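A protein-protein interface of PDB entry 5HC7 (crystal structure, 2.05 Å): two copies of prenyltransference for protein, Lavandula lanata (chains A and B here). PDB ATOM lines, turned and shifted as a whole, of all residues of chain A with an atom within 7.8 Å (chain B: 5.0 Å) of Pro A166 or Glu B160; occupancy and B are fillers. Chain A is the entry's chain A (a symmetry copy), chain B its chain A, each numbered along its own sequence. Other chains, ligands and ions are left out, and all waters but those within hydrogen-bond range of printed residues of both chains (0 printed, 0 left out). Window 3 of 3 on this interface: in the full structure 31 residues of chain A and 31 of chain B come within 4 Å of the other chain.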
ATOM      1  N   ILE A 155      -8.135  20.510 -27.872  1.00  0.00           N
ATOM      2  CA  ILE A 155      -8.106  21.966 -27.911  1.00  0.00           C
ATOM      3  C   ILE A 155      -6.765  22.430 -28.450  1.00  0.00           C
ATOM      4  O   ILE A 155      -6.686  23.441 -29.168  1.00  0.00           O
ATOM      5  CB  ILE A 155      -8.353  22.552 -26.534  1.00  0.00           C
ATOM      6  CG1 ILE A 155      -9.858  22.518 -26.222  1.00  0.00           C
ATOM      7  CG2 ILE A 155      -7.864  23.942 -26.427  1.00  0.00           C
ATOM      8  CD1 ILE A 155     -10.156  22.553 -24.721  1.00  0.00           C
ATOM      9  N   ALA A 156      -5.706  21.708 -28.095  1.00  0.00           N
ATOM     10  CA  ALA A 156      -4.367  22.051 -28.580  1.00  0.00           C
ATOM     11  C   ALA A 156      -4.245  21.825 -30.104  1.00  0.00           C
ATOM     12  O   ALA A 156      -3.677  22.661 -30.822  1.00  0.00           O
ATOM     13  CB  ALA A 156      -3.313  21.249 -27.813  1.00  0.00           C
ATOM     14  N   VAL A 159      -5.819  24.600 -31.746  1.00  0.00           N
ATOM     15  CA  VAL A 159      -4.993  25.788 -31.615  1.00  0.00           C
ATOM     16  C   VAL A 159      -3.936  25.707 -32.687  1.00  0.00           C
ATOM     17  O   VAL A 159      -3.587  26.718 -33.267  1.00  0.00           O
ATOM     18  CB  VAL A 159      -4.332  25.929 -30.221  1.00  0.00           C
ATOM     19  CG1 VAL A 159      -3.078  26.847 -30.224  1.00  0.00           C
ATOM     20  CG2 VAL A 159      -5.346  26.478 -29.228  1.00  0.00           C
ATOM     21  N   GLU A 160      -3.413  24.497 -32.899  1.00  0.00           N
ATOM     22  CA  GLU A 160      -2.344  24.286 -33.826  1.00  0.00           C
ATOM     23  C   GLU A 160      -2.848  24.576 -35.246  1.00  0.00           C
ATOM     24  O   GLU A 160      -2.091  25.030 -36.044  1.00  0.00           O
ATOM     25  CB  GLU A 160      -1.875  22.861 -33.739  1.00  0.00           C
ATOM     26  CG  GLU A 160      -0.711  22.504 -34.626  1.00  0.00           C
ATOM     27  CD  GLU A 160      -0.350  21.031 -34.575  1.00  0.00           C
ATOM     28  OE1 GLU A 160      -1.227  20.170 -34.805  1.00  0.00           O
ATOM     29  OE2 GLU A 160       0.827  20.741 -34.296  1.00  0.00           O
ATOM     30  N   GLY A 162      -4.896  26.913 -36.123  1.00  0.00           N
ATOM     31  CA  GLY A 162      -5.497  28.238 -36.146  1.00  0.00           C
ATOM     32  C   GLY A 162      -6.990  28.312 -35.905  1.00  0.00           C
ATOM     33  O   GLY A 162      -7.530  29.399 -35.858  1.00  0.00           O
ATOM     34  N   LEU A 164      -8.531  27.979 -33.187  1.00  0.00           N
ATOM     35  CA  LEU A 164      -8.781  28.488 -31.852  1.00  0.00           C
ATOM     36  C   LEU A 164      -7.526  29.179 -31.412  1.00  0.00           C
ATOM     37  O   LEU A 164      -6.429  28.664 -31.699  1.00  0.00           O
ATOM     38  CB  LEU A 164      -9.045  27.285 -30.933  1.00  0.00           C
ATOM     39  CG  LEU A 164     -10.134  27.288 -29.885  1.00  0.00           C
ATOM     40  CD1 LEU A 164     -11.497  27.627 -30.457  1.00  0.00           C
ATOM     41  CD2 LEU A 164     -10.180  25.912 -29.232  1.00  0.00           C
ATOM     42  N   ARG A 165      -7.654  30.292 -30.697  1.00  0.00           N
ATOM     43  CA  ARG A 165      -6.475  30.907 -30.078  1.00  0.00           C
ATOM     44  C   ARG A 165      -6.423  30.587 -28.555  1.00  0.00           C
ATOM     45  O   ARG A 165      -7.461  30.363 -27.923  1.00  0.00           O
ATOM     46  CB  ARG A 165      -6.498  32.421 -30.235  1.00  0.00           C
ATOM     47  CG  ARG A 165      -6.458  32.864 -31.702  1.00  0.00           C
ATOM     48  CD  ARG A 165      -6.949  34.279 -31.867  1.00  0.00           C
ATOM     49  NE  ARG A 165      -8.079  34.539 -30.970  1.00  0.00           N
ATOM     50  CZ  ARG A 165      -8.342  35.713 -30.402  1.00  0.00           C
ATOM     51  NH1 ARG A 165      -7.584  36.775 -30.647  1.00  0.00           N
ATOM     52  NH2 ARG A 165      -9.372  35.836 -29.584  1.00  0.00           N
ATOM     53  N   PRO A 166      -5.223  30.591 -27.963  1.00  0.00           N
ATOM     54  CA  PRO A 166      -5.096  30.331 -26.529  1.00  0.00           C
ATOM     55  C   PRO A 166      -6.038  31.137 -25.603  1.00  0.00           C
ATOM     56  O   PRO A 166      -6.689  30.546 -24.724  1.00  0.00           O
ATOM     57  CB  PRO A 166      -3.626  30.641 -26.278  1.00  0.00           C
ATOM     58  CG  PRO A 166      -2.994  30.094 -27.516  1.00  0.00           C
ATOM     59  CD  PRO A 166      -3.911  30.558 -28.623  1.00  0.00           C
ATOM     60  N   ASP A 167      -6.164  32.446 -25.815  1.00  0.00           N
ATOM     61  CA  ASP A 167      -7.095  33.202 -24.996  1.00  0.00           C
ATOM     62  C   ASP A 167      -8.558  32.990 -25.278  1.00  0.00           C
ATOM     63  O   ASP A 167      -9.371  33.449 -24.524  1.00  0.00           O
ATOM     64  CB  ASP A 167      -6.742  34.667 -24.929  1.00  0.00           C
ATOM     65  CG  ASP A 167      -5.550  34.918 -24.005  1.00  0.00           C
ATOM     66  OD1 ASP A 167      -4.817  33.945 -23.666  1.00  0.00           O
ATOM     67  OD2 ASP A 167      -5.337  36.093 -23.612  1.00  0.00           O
ATOM     68  N   ASP A 168      -8.909  32.213 -26.282  1.00  0.00           N
ATOM     69  CA  ASP A 168     -10.270  31.752 -26.402  1.00  0.00           C
ATOM     70  C   ASP A 168     -10.584  30.644 -25.429  1.00  0.00           C
ATOM     71  O   ASP A 168     -11.734  30.179 -25.422  1.00  0.00           O
ATOM     72  CB  ASP A 168     -10.596  31.145 -27.786  1.00  0.00           C
ATOM     73  CG  ASP A 168     -10.332  32.097 -28.970  1.00  0.00           C
ATOM     74  OD1 ASP A 168     -10.344  33.362 -28.792  1.00  0.00           O
ATOM     75  OD2 ASP A 168     -10.093  31.507 -30.076  1.00  0.00           O
ATOM     76  N   ILE A 169      -9.596  30.107 -24.706  1.00  0.00           N
ATOM     77  CA  ILE A 169      -9.929  28.913 -23.873  1.00  0.00           C
ATOM     78  C   ILE A 169     -10.588  29.360 -22.581  1.00  0.00           C
ATOM     79  O   ILE A 169     -10.006  30.056 -21.778  1.00  0.00           O
ATOM     80  CB  ILE A 169      -8.740  27.976 -23.625  1.00  0.00           C
ATOM     81  CG1 ILE A 169      -8.197  27.486 -24.976  1.00  0.00           C
ATOM     82  CG2 ILE A 169      -9.184  26.741 -22.892  1.00  0.00           C
ATOM     83  CD1 ILE A 169      -6.709  27.286 -24.944  1.00  0.00           C
ATOM     84  N   ASP A 170     -11.842  28.995 -22.416  1.00  0.00           N
ATOM     85  CA  ASP A 170     -12.483  29.271 -21.153  1.00  0.00           C
ATOM     86  C   ASP A 170     -13.151  27.992 -20.696  1.00  0.00           C
ATOM     87  O   ASP A 170     -13.077  26.955 -21.404  1.00  0.00           O
ATOM     88  CB  ASP A 170     -13.444  30.437 -21.339  1.00  0.00           C
ATOM     89  CG  ASP A 170     -14.542  30.143 -22.357  1.00  0.00           C
ATOM     90  OD1 ASP A 170     -14.676  29.007 -22.869  1.00  0.00           O
ATOM     91  OD2 ASP A 170     -15.309  31.081 -22.641  1.00  0.00           O
ATOM     92  N   THR A 173     -15.438  26.454 -23.242  1.00  0.00           N
ATOM     93  CA  THR A 173     -14.740  25.794 -24.323  1.00  0.00           C
ATOM     94  C   THR A 173     -14.204  24.466 -23.859  1.00  0.00           C
ATOM     95  O   THR A 173     -14.312  23.411 -24.509  1.00  0.00           O
ATOM     96  CB  THR A 173     -13.583  26.696 -24.802  1.00  0.00           C
ATOM     97  OG1 THR A 173     -14.155  27.934 -25.229  1.00  0.00           O
ATOM     98  CG2 THR A 173     -12.879  26.037 -25.971  1.00  0.00           C
ATOM     99  N   ARG B 153      -4.614  26.884 -21.028  1.00  0.00           N
ATOM    100  CA  ARG B 153      -4.236  28.073 -21.764  1.00  0.00           C
ATOM    101  C   ARG B 153      -2.729  28.165 -21.939  1.00  0.00           C
ATOM    102  O   ARG B 153      -2.255  28.400 -23.045  1.00  0.00           O
ATOM    103  CB  ARG B 153      -4.665  29.303 -21.007  1.00  0.00           C
ATOM    104  CG  ARG B 153      -6.083  29.717 -21.204  1.00  0.00           C
ATOM    105  CD  ARG B 153      -6.301  31.030 -20.479  1.00  0.00           C
ATOM    106  NE  ARG B 153      -7.718  31.253 -20.288  1.00  0.00           N
ATOM    107  CZ  ARG B 153      -8.434  32.163 -20.929  1.00  0.00           C
ATOM    108  NH1 ARG B 153      -7.855  32.966 -21.825  1.00  0.00           N
ATOM    109  NH2 ARG B 153      -9.738  32.273 -20.656  1.00  0.00           N
ATOM    110  N   ALA B 156      -1.630  25.702 -24.444  1.00  0.00           N
ATOM    111  CA  ALA B 156      -2.052  26.097 -25.790  1.00  0.00           C
ATOM    112  C   ALA B 156      -1.117  27.176 -26.380  1.00  0.00           C
ATOM    113  O   ALA B 156      -0.736  27.105 -27.558  1.00  0.00           O
ATOM    114  CB  ALA B 156      -3.505  26.578 -25.760  1.00  0.00           C
ATOM    115  N   ALA B 157      -0.728  28.143 -25.551  1.00  0.00           N
ATOM    116  CA  ALA B 157       0.245  29.136 -25.983  1.00  0.00           C
ATOM    117  C   ALA B 157       1.550  28.504 -26.424  1.00  0.00           C
ATOM    118  O   ALA B 157       2.182  28.963 -27.370  1.00  0.00           O
ATOM    119  CB  ALA B 157       0.550  30.090 -24.861  1.00  0.00           C
ATOM    120  N   LYS B 158       1.971  27.473 -25.689  1.00  0.00           N
ATOM    121  CA  LYS B 158       3.222  26.791 -25.976  1.00  0.00           C
ATOM    122  C   LYS B 158       3.073  26.007 -27.251  1.00  0.00           C
ATOM    123  O   LYS B 158       4.042  25.849 -27.972  1.00  0.00           O
ATOM    124  CB  LYS B 158       3.681  25.858 -24.830  1.00  0.00           C
ATOM    125  CG  LYS B 158       4.160  26.514 -23.547  1.00  0.00           C
ATOM    126  CD  LYS B 158       4.901  25.408 -22.793  1.00  0.00           C
ATOM    127  CE  LYS B 158       5.522  25.887 -21.485  1.00  0.00           C
ATOM    128  NZ  LYS B 158       6.279  24.756 -20.883  1.00  0.00           N
ATOM    129  N   VAL B 159       1.855  25.527 -27.530  1.00  0.00           N
ATOM    130  CA  VAL B 159       1.569  24.774 -28.739  1.00  0.00           C
ATOM    131  C   VAL B 159       1.623  25.750 -29.887  1.00  0.00           C
ATOM    132  O   VAL B 159       2.098  25.403 -30.952  1.00  0.00           O
ATOM    133  CB  VAL B 159       0.195  24.059 -28.709  1.00  0.00           C
ATOM    134  CG1 VAL B 159      -0.349  23.711 -30.122  1.00  0.00           C
ATOM    135  CG2 VAL B 159       0.303  22.780 -27.892  1.00  0.00           C
ATOM    136  N   GLU B 160       1.090  26.951 -29.655  1.00  0.00           N
ATOM    137  CA  GLU B 160       0.997  27.949 -30.677  1.00  0.00           C
ATOM    138  C   GLU B 160       2.411  28.391 -31.075  1.00  0.00           C
ATOM    139  O   GLU B 160       2.617  28.714 -32.201  1.00  0.00           O
ATOM    140  CB  GLU B 160       0.225  29.130 -30.159  1.00  0.00           C
ATOM    141  CG  GLU B 160       0.001  30.243 -31.149  1.00  0.00           C
ATOM    142  CD  GLU B 160      -0.689  31.452 -30.542  1.00  0.00           C
ATOM    143  OE1 GLU B 160      -0.206  31.995 -29.525  1.00  0.00           O
ATOM    144  OE2 GLU B 160      -1.729  31.853 -31.095  1.00  0.00           O
ATOM    145  N   HIS B 161       3.376  28.395 -30.162  1.00  0.00           N
ATOM    146  CA  HIS B 161       4.722  28.819 -30.495  1.00  0.00           C
ATOM    147  C   HIS B 161       5.587  27.626 -30.886  1.00  0.00           C
ATOM    148  O   HIS B 161       6.765  27.710 -30.765  1.00  0.00           O
ATOM    149  CB  HIS B 161       5.374  29.543 -29.308  1.00  0.00           C
ATOM    150  CG  HIS B 161       4.800  30.894 -29.026  1.00  0.00           C
ATOM    151  ND1 HIS B 161       3.445  31.166 -29.089  1.00  0.00           N
ATOM    152  CD2 HIS B 161       5.395  32.051 -28.652  1.00  0.00           C
ATOM    153  CE1 HIS B 161       3.234  32.434 -28.783  1.00  0.00           C
ATOM    154  NE2 HIS B 161       4.401  32.995 -28.519  1.00  0.00           N
ATOM    155  N   GLY B 162       5.022  26.507 -31.322  1.00  0.00           N
ATOM    156  CA  GLY B 162       5.804  25.329 -31.662  1.00  0.00           C
ATOM    157  C   GLY B 162       6.619  24.708 -30.546  1.00  0.00           C
ATOM    158  O   GLY B 162       7.244  23.690 -30.764  1.00  0.00           O
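Hydrophobic or aromatic side chains of chain A that line the printed part of chain B: Ala A156, Val A159, Pro A166 and Ile A169. Along chain A the printed residues that touch a printed residue of chain B span positions 156 to 169. Hydrophobic or aromatic side chains of chain B within 4 Å of the printed part of chain A: Ala B156 and Val B159.
The backbone carbonyl oxygen (O) of Ala B157 lies within hydrogen-bond range of a ring nitrogen (ND1) of His B161, 3.1 Å away.
Among the printed residues, merely in contact across the chains: Ile A169 with Ala B156 (3.4 Å), Pro A166 with Glu B160 (3.5 Å), Val A159 with Ala B156 (3.6 Å), Ala A156 with Val B159 (3.6 Å), Pro A166 with Ala B157 (3.6 Å), Pro A166 with Ala B156 (3.7 Å) and Pro A166 with Arg B153 (3.7 Å).
Ala A156 touches Val B159, and with the chains exchanged Val A159 touches Ala B156. Positions printed for both chains: 156, 159, 160 and 162.
NH1 of Arg B153 lies within salt-bridge range of OD1 of Asp A167 (3.7 Å). The backbone carbonyl oxygen (O) of Ile A169 is in hydrogen-bond range of the guanidinium group (NH2) of Arg B153 (2.5 Å).
Of the printed residues of chain B, Val A159 touches Ala B156 (3.6 Å). Of chain B, only Arg B153, Ala B156, Ala B157 and Glu B160 come within 4 Å of Pro A166. Printed residues of chain B within 4 Å of Asp A167: Arg B153. Of the printed residues of chain A, Glu B160 touches Pro A166. The nearest printed residue of chain A that does not touch Glu B160 is Val A159 (4.02 Å). The nearest printed residue of chain A that does not touch Val B159 is Glu A160 (4.02 Å).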
